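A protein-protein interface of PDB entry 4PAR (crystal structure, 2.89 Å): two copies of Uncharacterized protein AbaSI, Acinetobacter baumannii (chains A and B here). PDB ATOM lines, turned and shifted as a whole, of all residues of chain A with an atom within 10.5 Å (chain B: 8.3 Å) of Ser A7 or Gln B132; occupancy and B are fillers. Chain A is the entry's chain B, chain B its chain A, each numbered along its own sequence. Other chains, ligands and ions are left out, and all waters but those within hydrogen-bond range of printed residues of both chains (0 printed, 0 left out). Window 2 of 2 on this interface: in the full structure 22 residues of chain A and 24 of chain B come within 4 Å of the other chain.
No position is printed for both chains.
O of Gln B134 lies within hydrogen-bond range of OG1 of Thr A10, 2.6 Å away. The backbone NH (N) of Leu B136 is in hydrogen-bond range of the side-chain hydroxyl (OG1) of Thr A10, at 3.3 Å. The guanidinium group (NH2) of Arg B24 is in salt-bridge range of the side-chain carboxylate (OD1) of Asp A11 (2.7 Å).
Ser A6 touches Asn B135. Ser A7 touches Gln B132 (OG to OE1, 3.5 Å). Pro B133 touches Ser A7 (O to CB, 3.3 Å). CG of Leu A9 touches CD1 of Leu B136, at 3.8 Å. Thr A10 touches Tyr B25 (CG2 to CE2, 3.9 Å). Asn B135 touches Thr A10. Val A13 touches Leu B136. CG1 of Ile A14 touches CE2 of Tyr B25, at 3.7 Å.
The backbone carbonyl oxygen (O) of Val B125 is in hydrogen-bond range of the backbone NH (N) of Gln B134 (3.1 Å).
Hydrophobic or aromatic side chains of chain B that line the printed part of chain A: Tyr B25, Pro B133 and Leu B136. Hydrophobic or aromatic side chains of chain A within 4 Å of the printed part of chain B: Leu A9, Val A13 and Ile A14. Among the printed residues, Asp or Glu carboxylates within 4 Å of a Lys or Arg side-chain nitrogen of the other chain: Asp A11 with Arg B24 (2.7 Å).
Of chain B, only Gln B132 (3.5 Å) and Pro B133 (3.3 Å) come within 4 Å of Ser A7. Of chain A, only Ser A7 (3.5 Å) comes within 4 Å of Gln B132. No residue of chain A comes within 4 Å of Phe B126. No residue of chain A comes within 4 Å of Lys B127. Gly B131 touches none of the printed residues of chain A. Printed residues of chain B within 4 Å of Ser A6: Asn B135. Of the printed residues of chain A, Gln B134 touches Thr A10. Of the printed residues of chain B, Leu A9 touches Leu B136 (3.8 Å). Of the printed residues of chain B, Asp A11 touches Arg B24. Of the printed residues of chain A, Tyr B25 touches Thr A10 and Ile A14. Glu B130 touches none of the printed residues of chain A. The nearest residue of chain B that does not touch Ser A7 is Gln B134 (4.2 Å). The nearest printed residue of chain A that does not touch Leu B136 is Ser A6 (5.1 Å).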
ATOM      1  N   ALA A   5     -18.080 -30.291  14.965  1.00  0.00           N
ATOM      2  CA  ALA A   5     -18.460 -29.254  14.011  1.00  0.00           C
ATOM      3  C   ALA A   5     -17.231 -28.680  13.314  1.00  0.00           C
ATOM      4  O   ALA A   5     -16.577 -29.367  12.533  1.00  0.00           O
ATOM      5  CB  ALA A   5     -19.244 -28.149  14.710  1.00  0.00           C
ATOM      6  N   SER A   6     -16.913 -27.421  13.593  1.00  0.00           N
ATOM      7  CA  SER A   6     -15.722 -26.797  13.023  1.00  0.00           C
ATOM      8  C   SER A   6     -14.475 -27.273  13.770  1.00  0.00           C
ATOM      9  O   SER A   6     -13.339 -27.198  13.269  1.00  0.00           O
ATOM     10  CB  SER A   6     -15.834 -25.273  13.084  1.00  0.00           C
ATOM     11  OG  SER A   6     -17.111 -24.827  12.663  1.00  0.00           O
ATOM     12  N   SER A   7     -14.709 -27.757  14.984  1.00  0.00           N
ATOM     13  CA  SER A   7     -13.657 -28.285  15.833  1.00  0.00           C
ATOM     14  C   SER A   7     -12.943 -29.446  15.162  1.00  0.00           C
ATOM     15  O   SER A   7     -11.755 -29.661  15.389  1.00  0.00           O
ATOM     16  CB  SER A   7     -14.230 -28.735  17.178  1.00  0.00           C
ATOM     17  OG  SER A   7     -15.098 -29.843  17.024  1.00  0.00           O
ATOM     18  N   ASP A   8     -13.673 -30.198  14.345  1.00  0.00           N
ATOM     19  CA  ASP A   8     -13.082 -31.303  13.600  1.00  0.00           C
ATOM     20  C   ASP A   8     -12.023 -30.783  12.638  1.00  0.00           C
ATOM     21  O   ASP A   8     -10.937 -31.353  12.533  1.00  0.00           O
ATOM     22  CB  ASP A   8     -14.162 -32.085  12.848  1.00  0.00           C
ATOM     23  CG  ASP A   8     -15.059 -32.880  13.780  1.00  0.00           C
ATOM     24  OD1 ASP A   8     -16.020 -32.297  14.330  1.00  0.00           O
ATOM     25  OD2 ASP A   8     -14.798 -34.088  13.965  1.00  0.00           O
ATOM     26  N   LEU A   9     -12.344 -29.691  11.951  1.00  0.00           N
ATOM     27  CA  LEU A   9     -11.375 -29.014  11.101  1.00  0.00           C
ATOM     28  C   LEU A   9     -10.161 -28.598  11.915  1.00  0.00           C
ATOM     29  O   LEU A   9      -9.022 -28.863  11.516  1.00  0.00           O
ATOM     30  CB  LEU A   9     -11.990 -27.787  10.426  1.00  0.00           C
ATOM     31  CG  LEU A   9     -10.968 -26.891   9.722  1.00  0.00           C
ATOM     32  CD1 LEU A   9     -10.317 -27.647   8.580  1.00  0.00           C
ATOM     33  CD2 LEU A   9     -11.596 -25.607   9.219  1.00  0.00           C
ATOM     34  N   THR A  10     -10.407 -27.954  13.057  1.00  0.00           N
ATOM     35  CA  THR A  10      -9.300 -27.526  13.920  1.00  0.00           C
ATOM     36  C   THR A  10      -8.345 -28.681  14.249  1.00  0.00           C
ATOM     37  O   THR A  10      -7.144 -28.619  13.944  1.00  0.00           O
ATOM     38  CB  THR A  10      -9.811 -26.923  15.240  1.00  0.00           C
ATOM     39  OG1 THR A  10     -10.606 -25.763  14.964  1.00  0.00           O
ATOM     40  CG2 THR A  10      -8.651 -26.537  16.140  1.00  0.00           C
ATOM     41  N   ASP A  11      -8.895 -29.740  14.840  1.00  0.00           N
ATOM     42  CA  ASP A  11      -8.125 -30.934  15.192  1.00  0.00           C
ATOM     43  C   ASP A  11      -7.358 -31.493  13.993  1.00  0.00           C
ATOM     44  O   ASP A  11      -6.175 -31.810  14.097  1.00  0.00           O
ATOM     45  CB  ASP A  11      -9.053 -32.010  15.767  1.00  0.00           C
ATOM     46  CG  ASP A  11      -8.308 -33.270  16.178  1.00  0.00           C
ATOM     47  OD1 ASP A  11      -7.778 -33.314  17.311  1.00  0.00           O
ATOM     48  OD2 ASP A  11      -8.264 -34.220  15.369  1.00  0.00           O
ATOM     49  N   TYR A  12      -8.039 -31.601  12.857  1.00  0.00           N
ATOM     50  CA  TYR A  12      -7.438 -32.164  11.655  1.00  0.00           C
ATOM     51  C   TYR A  12      -6.206 -31.367  11.217  1.00  0.00           C
ATOM     52  O   TYR A  12      -5.125 -31.936  11.010  1.00  0.00           O
ATOM     53  CB  TYR A  12      -8.474 -32.221  10.527  1.00  0.00           C
ATOM     54  CG  TYR A  12      -7.915 -32.662   9.192  1.00  0.00           C
ATOM     55  CD1 TYR A  12      -7.717 -34.006   8.909  1.00  0.00           C
ATOM     56  CD2 TYR A  12      -7.588 -31.731   8.213  1.00  0.00           C
ATOM     57  CE1 TYR A  12      -7.202 -34.405   7.691  1.00  0.00           C
ATOM     58  CE2 TYR A  12      -7.078 -32.124   6.997  1.00  0.00           C
ATOM     59  CZ  TYR A  12      -6.887 -33.459   6.743  1.00  0.00           C
ATOM     60  OH  TYR A  12      -6.380 -33.848   5.528  1.00  0.00           O
ATOM     61  N   VAL A  13      -6.369 -30.053  11.092  1.00  0.00           N
ATOM     62  CA  VAL A  13      -5.252 -29.168  10.759  1.00  0.00           C
ATOM     63  C   VAL A  13      -4.083 -29.299  11.740  1.00  0.00           C
ATOM     64  O   VAL A  13      -2.926 -29.501  11.319  1.00  0.00           O
ATOM     65  CB  VAL A  13      -5.693 -27.695  10.726  1.00  0.00           C
ATOM     66  CG1 VAL A  13      -4.502 -26.807  10.452  1.00  0.00           C
ATOM     67  CG2 VAL A  13      -6.763 -27.487   9.666  1.00  0.00           C
ATOM     68  N   ILE A  14      -4.386 -29.186  13.035  1.00  0.00           N
ATOM     69  CA  ILE A  14      -3.357 -29.324  14.067  1.00  0.00           C
ATOM     70  C   ILE A  14      -2.572 -30.616  13.896  1.00  0.00           C
ATOM     71  O   ILE A  14      -1.343 -30.611  13.908  1.00  0.00           O
ATOM     72  CB  ILE A  14      -3.957 -29.301  15.489  1.00  0.00           C
ATOM     73  CG1 ILE A  14      -4.572 -27.941  15.779  1.00  0.00           C
ATOM     74  CG2 ILE A  14      -2.900 -29.620  16.531  1.00  0.00           C
ATOM     75  CD1 ILE A  14      -3.641 -26.815  15.501  1.00  0.00           C
ATOM     76  N   ARG A  15      -3.292 -31.717  13.716  1.00  0.00           N
ATOM     77  CA  ARG A  15      -2.662 -33.023  13.617  1.00  0.00           C
ATOM     78  C   ARG A  15      -1.804 -33.143  12.360  1.00  0.00           C
ATOM     79  O   ARG A  15      -0.736 -33.751  12.399  1.00  0.00           O
ATOM     80  CB  ARG A  15      -3.722 -34.128  13.657  1.00  0.00           C
ATOM     81  CG  ARG A  15      -4.417 -34.250  15.015  1.00  0.00           C
ATOM     82  CD  ARG A  15      -5.354 -35.440  15.066  1.00  0.00           C
ATOM     83  NE  ARG A  15      -4.637 -36.702  14.919  1.00  0.00           N
ATOM     84  CZ  ARG A  15      -5.222 -37.894  14.885  1.00  0.00           C
ATOM     85  NH1 ARG A  15      -6.541 -37.989  14.986  1.00  0.00           N
ATOM     86  NH2 ARG A  15      -4.489 -38.993  14.749  1.00  0.00           N
ATOM     87  N   TRP A 166     -14.430 -28.029   0.548  1.00  0.00           N
ATOM     88  CA  TRP A 166     -14.124 -29.087   1.488  1.00  0.00           C
ATOM     89  C   TRP A 166     -14.983 -28.994   2.739  1.00  0.00           C
ATOM     90  O   TRP A 166     -14.960 -27.983   3.440  1.00  0.00           O
ATOM     91  CB  TRP A 166     -12.645 -29.029   1.857  1.00  0.00           C
ATOM     92  CG  TRP A 166     -12.241 -29.996   2.912  1.00  0.00           C
ATOM     93  CD1 TRP A 166     -12.746 -31.247   3.122  1.00  0.00           C
ATOM     94  CD2 TRP A 166     -11.245 -29.790   3.915  1.00  0.00           C
ATOM     95  NE1 TRP A 166     -12.119 -31.834   4.195  1.00  0.00           N
ATOM     96  CE2 TRP A 166     -11.194 -30.958   4.701  1.00  0.00           C
ATOM     97  CE3 TRP A 166     -10.388 -28.731   4.225  1.00  0.00           C
ATOM     98  CZ2 TRP A 166     -10.321 -31.095   5.775  1.00  0.00           C
ATOM     99  CZ3 TRP A 166      -9.523 -28.868   5.290  1.00  0.00           C
ATOM    100  CH2 TRP A 166      -9.495 -30.040   6.053  1.00  0.00           C
ATOM    101  N   ASN A 167     -15.746 -30.046   3.016  1.00  0.00           N
ATOM    102  CA  ASN A 167     -16.510 -30.108   4.254  1.00  0.00           C
ATOM    103  C   ASN A 167     -16.277 -31.407   5.019  1.00  0.00           C
ATOM    104  O   ASN A 167     -16.638 -32.482   4.544  1.00  0.00           O
ATOM    105  CB  ASN A 167     -18.002 -29.938   3.975  1.00  0.00           C
ATOM    106  CG  ASN A 167     -18.810 -29.758   5.246  1.00  0.00           C
ATOM    107  OD1 ASN A 167     -19.199 -30.731   5.892  1.00  0.00           O
ATOM    108  ND2 ASN A 167     -19.054 -28.507   5.619  1.00  0.00           N
ATOM    109  N   ILE A 168     -15.683 -31.292   6.207  1.00  0.00           N
ATOM    110  CA  ILE A 168     -15.413 -32.438   7.073  1.00  0.00           C
ATOM    111  C   ILE A 168     -16.641 -33.302   7.299  1.00  0.00           C
ATOM    112  O   ILE A 168     -16.573 -34.527   7.195  1.00  0.00           O
ATOM    113  CB  ILE A 168     -14.897 -31.993   8.454  1.00  0.00           C
ATOM    114  CG1 ILE A 168     -13.468 -31.474   8.359  1.00  0.00           C
ATOM    115  CG2 ILE A 168     -14.930 -33.157   9.431  1.00  0.00           C
ATOM    116  CD1 ILE A 168     -12.437 -32.578   8.282  1.00  0.00           C
ATOM    117  N   GLU A 169     -17.762 -32.656   7.603  1.00  0.00           N
ATOM    118  CA  GLU A 169     -18.966 -33.362   8.029  1.00  0.00           C
ATOM    119  C   GLU A 169     -19.602 -34.169   6.904  1.00  0.00           C
ATOM    120  O   GLU A 169     -20.095 -35.276   7.127  1.00  0.00           O
ATOM    121  CB  GLU A 169     -19.986 -32.373   8.596  1.00  0.00           C
ATOM    122  CG  GLU A 169     -19.419 -31.438   9.660  1.00  0.00           C
ATOM    123  CD  GLU A 169     -18.900 -32.179  10.880  1.00  0.00           C
ATOM    124  OE1 GLU A 169     -19.538 -33.170  11.295  1.00  0.00           O
ATOM    125  OE2 GLU A 169     -17.851 -31.770  11.422  1.00  0.00           O
ATOM    126  N   ARG B  24       0.311 -28.959  23.135  1.00  0.00           N
ATOM    127  CA  ARG B  24      -0.273 -29.513  21.917  1.00  0.00           C
ATOM    128  C   ARG B  24      -0.521 -28.478  20.817  1.00  0.00           C
ATOM    129  O   ARG B  24      -0.246 -28.730  19.643  1.00  0.00           O
ATOM    130  CB  ARG B  24      -1.584 -30.217  22.268  1.00  0.00           C
ATOM    131  CG  ARG B  24      -2.362 -30.742  21.082  1.00  0.00           C
ATOM    132  CD  ARG B  24      -3.351 -31.790  21.531  1.00  0.00           C
ATOM    133  NE  ARG B  24      -4.574 -31.760  20.738  1.00  0.00           N
ATOM    134  CZ  ARG B  24      -4.783 -32.509  19.662  1.00  0.00           C
ATOM    135  NH1 ARG B  24      -3.844 -33.350  19.248  1.00  0.00           N
ATOM    136  NH2 ARG B  24      -5.934 -32.416  19.003  1.00  0.00           N
ATOM    137  N   TYR B  25      -1.050 -27.321  21.197  1.00  0.00           N
ATOM    138  CA  TYR B  25      -1.369 -26.264  20.241  1.00  0.00           C
ATOM    139  C   TYR B  25      -0.271 -25.205  20.114  1.00  0.00           C
ATOM    140  O   TYR B  25      -0.475 -24.178  19.464  1.00  0.00           O
ATOM    141  CB  TYR B  25      -2.695 -25.606  20.616  1.00  0.00           C
ATOM    142  CG  TYR B  25      -3.895 -26.438  20.222  1.00  0.00           C
ATOM    143  CD1 TYR B  25      -4.089 -27.707  20.751  1.00  0.00           C
ATOM    144  CD2 TYR B  25      -4.830 -25.957  19.318  1.00  0.00           C
ATOM    145  CE1 TYR B  25      -5.178 -28.475  20.390  1.00  0.00           C
ATOM    146  CE2 TYR B  25      -5.925 -26.720  18.952  1.00  0.00           C
ATOM    147  CZ  TYR B  25      -6.093 -27.978  19.490  1.00  0.00           C
ATOM    148  OH  TYR B  25      -7.182 -28.740  19.131  1.00  0.00           O
ATOM    149  N   HIS B  78      -4.228 -30.541  30.355  1.00  0.00           N
ATOM    150  CA  HIS B  78      -3.990 -31.815  29.723  1.00  0.00           C
ATOM    151  C   HIS B  78      -2.567 -32.018  29.342  1.00  0.00           C
ATOM    152  O   HIS B  78      -2.062 -33.147  29.297  1.00  0.00           O
ATOM    153  CB  HIS B  78      -4.861 -31.941  28.507  1.00  0.00           C
ATOM    154  CG  HIS B  78      -6.218 -31.332  28.674  1.00  0.00           C
ATOM    155  ND1 HIS B  78      -7.328 -32.069  28.770  1.00  0.00           N
ATOM    156  CD2 HIS B  78      -6.614 -30.012  28.747  1.00  0.00           C
ATOM    157  CE1 HIS B  78      -8.384 -31.261  28.894  1.00  0.00           C
ATOM    158  NE2 HIS B  78      -7.946 -30.003  28.882  1.00  0.00           N
ATOM    159  N   VAL B 125      -7.458 -21.996  23.342  1.00  0.00           N
ATOM    160  CA  VAL B 125      -7.652 -22.930  22.247  1.00  0.00           C
ATOM    161  C   VAL B 125      -8.822 -23.889  22.441  1.00  0.00           C
ATOM    162  O   VAL B 125      -9.119 -24.693  21.562  1.00  0.00           O
ATOM    163  CB  VAL B 125      -6.387 -23.747  22.031  1.00  0.00           C
ATOM    164  CG1 VAL B 125      -5.222 -22.818  21.735  1.00  0.00           C
ATOM    165  CG2 VAL B 125      -6.105 -24.587  23.262  1.00  0.00           C
ATOM    166  N   PHE B 126      -9.492 -23.805  23.586  1.00  0.00           N
ATOM    167  CA  PHE B 126     -10.608 -24.703  23.857  1.00  0.00           C
ATOM    168  C   PHE B 126     -11.890 -23.937  24.147  1.00  0.00           C
ATOM    169  O   PHE B 126     -11.914 -23.057  25.008  1.00  0.00           O
ATOM    170  CB  PHE B 126     -10.277 -25.630  25.027  1.00  0.00           C
ATOM    171  CG  PHE B 126      -9.142 -26.571  24.750  1.00  0.00           C
ATOM    172  CD1 PHE B 126      -8.954 -27.099  23.488  1.00  0.00           C
ATOM    173  CD2 PHE B 126      -8.258 -26.924  25.751  1.00  0.00           C
ATOM    174  CE1 PHE B 126      -7.908 -27.963  23.233  1.00  0.00           C
ATOM    175  CE2 PHE B 126      -7.216 -27.785  25.507  1.00  0.00           C
ATOM    176  CZ  PHE B 126      -7.036 -28.305  24.246  1.00  0.00           C
ATOM    177  N   LYS B 127     -12.953 -24.272  23.422  1.00  0.00           N
ATOM    178  CA  LYS B 127     -14.253 -23.668  23.670  1.00  0.00           C
ATOM    179  C   LYS B 127     -14.849 -24.273  24.940  1.00  0.00           C
ATOM    180  O   LYS B 127     -14.941 -23.606  25.970  1.00  0.00           O
ATOM    181  CB  LYS B 127     -15.196 -23.854  22.469  1.00  0.00           C
ATOM    182  CG  LYS B 127     -15.185 -25.235  21.819  1.00  0.00           C
ATOM    183  CD  LYS B 127     -16.397 -25.428  20.909  1.00  0.00           C
ATOM    184  CE  LYS B 127     -16.507 -26.866  20.413  1.00  0.00           C
ATOM    185  NZ  LYS B 127     -17.753 -27.082  19.628  1.00  0.00           N
ATOM    186  N   ASN B 128     -15.225 -25.546  24.873  1.00  0.00           N
ATOM    187  CA  ASN B 128     -15.676 -26.258  26.053  1.00  0.00           C
ATOM    188  C   ASN B 128     -14.536 -27.113  26.565  1.00  0.00           C
ATOM    189  O   ASN B 128     -14.204 -28.135  25.971  1.00  0.00           O
ATOM    190  CB  ASN B 128     -16.892 -27.136  25.741  1.00  0.00           C
ATOM    191  CG  ASN B 128     -18.078 -26.340  25.226  1.00  0.00           C
ATOM    192  OD1 ASN B 128     -18.274 -26.208  24.016  1.00  0.00           O
ATOM    193  ND2 ASN B 128     -18.886 -25.819  26.144  1.00  0.00           N
ATOM    194  N   GLN B 129     -13.945 -26.695  27.675  1.00  0.00           N
ATOM    195  CA  GLN B 129     -12.872 -27.450  28.298  1.00  0.00           C
ATOM    196  C   GLN B 129     -13.416 -28.126  29.552  1.00  0.00           C
ATOM    197  O   GLN B 129     -14.187 -27.516  30.292  1.00  0.00           O
ATOM    198  CB  GLN B 129     -11.688 -26.534  28.614  1.00  0.00           C
ATOM    199  CG  GLN B 129     -10.997 -26.818  29.934  1.00  0.00           C
ATOM    200  CD  GLN B 129      -9.495 -26.841  29.795  1.00  0.00           C
ATOM    201  OE1 GLN B 129      -8.972 -27.195  28.740  1.00  0.00           O
ATOM    202  NE2 GLN B 129      -8.790 -26.460  30.856  1.00  0.00           N
ATOM    203  N   GLU B 130     -13.037 -29.379  29.803  1.00  0.00           N
ATOM    204  CA  GLU B 130     -12.041 -30.123  29.034  1.00  0.00           C
ATOM    205  C   GLU B 130     -12.560 -30.659  27.695  1.00  0.00           C
ATOM    206  O   GLU B 130     -13.723 -30.445  27.343  1.00  0.00           O
ATOM    207  CB  GLU B 130     -11.511 -31.283  29.884  1.00  0.00           C
ATOM    208  CG  GLU B 130     -12.576 -32.048  30.665  1.00  0.00           C
ATOM    209  CD  GLU B 130     -12.919 -31.398  32.000  1.00  0.00           C
ATOM    210  OE1 GLU B 130     -12.171 -30.498  32.439  1.00  0.00           O
ATOM    211  OE2 GLU B 130     -13.941 -31.784  32.607  1.00  0.00           O
ATOM    212  N   GLY B 131     -11.715 -31.403  26.981  1.00  0.00           N
ATOM    213  CA  GLY B 131     -12.049 -31.846  25.637  1.00  0.00           C
ATOM    214  C   GLY B 131     -12.024 -30.801  24.530  1.00  0.00           C
ATOM    215  O   GLY B 131     -10.974 -30.219  24.232  1.00  0.00           O
ATOM    216  N   GLN B 132     -13.190 -30.580  23.925  1.00  0.00           N
ATOM    217  CA  GLN B 132     -13.350 -29.976  22.598  1.00  0.00           C
ATOM    218  C   GLN B 132     -12.503 -28.743  22.290  1.00  0.00           C
ATOM    219  O   GLN B 132     -12.412 -27.821  23.094  1.00  0.00           O
ATOM    220  CB  GLN B 132     -14.818 -29.582  22.403  1.00  0.00           C
ATOM    221  CG  GLN B 132     -15.814 -30.709  22.573  1.00  0.00           C
ATOM    222  CD  GLN B 132     -16.099 -31.416  21.272  1.00  0.00           C
ATOM    223  OE1 GLN B 132     -15.430 -31.176  20.264  1.00  0.00           O
ATOM    224  NE2 GLN B 132     -17.099 -32.290  21.279  1.00  0.00           N
ATOM    225  N   PRO B 133     -11.875 -28.739  21.106  1.00  0.00           N
ATOM    226  CA  PRO B 133     -11.137 -27.591  20.577  1.00  0.00           C
ATOM    227  C   PRO B 133     -12.093 -26.530  20.050  1.00  0.00           C
ATOM    228  O   PRO B 133     -13.245 -26.849  19.749  1.00  0.00           O
ATOM    229  CB  PRO B 133     -10.310 -28.192  19.429  1.00  0.00           C
ATOM    230  CG  PRO B 133     -10.585 -29.688  19.453  1.00  0.00           C
ATOM    231  CD  PRO B 133     -11.886 -29.857  20.152  1.00  0.00           C
ATOM    232  N   GLN B 134     -11.628 -25.291  19.932  1.00  0.00           N
ATOM    233  CA  GLN B 134     -12.464 -24.237  19.374  1.00  0.00           C
ATOM    234  C   GLN B 134     -12.343 -24.202  17.856  1.00  0.00           C
ATOM    235  O   GLN B 134     -11.580 -24.968  17.269  1.00  0.00           O
ATOM    236  CB  GLN B 134     -12.089 -22.882  19.970  1.00  0.00           C
ATOM    237  CG  GLN B 134     -13.273 -21.938  20.110  1.00  0.00           C
ATOM    238  CD  GLN B 134     -12.899 -20.635  20.772  1.00  0.00           C
ATOM    239  OE1 GLN B 134     -11.728 -20.387  21.060  1.00  0.00           O
ATOM    240  NE2 GLN B 134     -13.892 -19.790  21.017  1.00  0.00           N
ATOM    241  N   ASN B 135     -13.101 -23.313  17.220  1.00  0.00           N
ATOM    242  CA  ASN B 135     -13.058 -23.172  15.770  1.00  0.00           C
ATOM    243  C   ASN B 135     -11.889 -22.298  15.341  1.00  0.00           C
ATOM    244  O   ASN B 135     -11.561 -21.313  16.009  1.00  0.00           O
ATOM    245  CB  ASN B 135     -14.371 -22.596  15.241  1.00  0.00           C
ATOM    246  CG  ASN B 135     -14.740 -21.285  15.904  1.00  0.00           C
ATOM    247  OD1 ASN B 135     -14.163 -20.240  15.603  1.00  0.00           O
ATOM    248  ND2 ASN B 135     -15.712 -21.332  16.809  1.00  0.00           N
ATOM    249  N   LEU B 136     -11.269 -22.667  14.224  1.00  0.00           N
ATOM    250  CA  LEU B 136     -10.064 -22.003  13.736  1.00  0.00           C
ATOM    251  C   LEU B 136     -10.221 -20.501  13.548  1.00  0.00           C
ATOM    252  O   LEU B 136      -9.263 -19.751  13.721  1.00  0.00           O
ATOM    253  CB  LEU B 136      -9.621 -22.630  12.415  1.00  0.00           C
ATOM    254  CG  LEU B 136      -8.848 -23.940  12.522  1.00  0.00           C
ATOM    255  CD1 LEU B 136      -8.504 -24.437  11.144  1.00  0.00           C
ATOM    256  CD2 LEU B 136      -7.596 -23.732  13.338  1.00  0.00           C
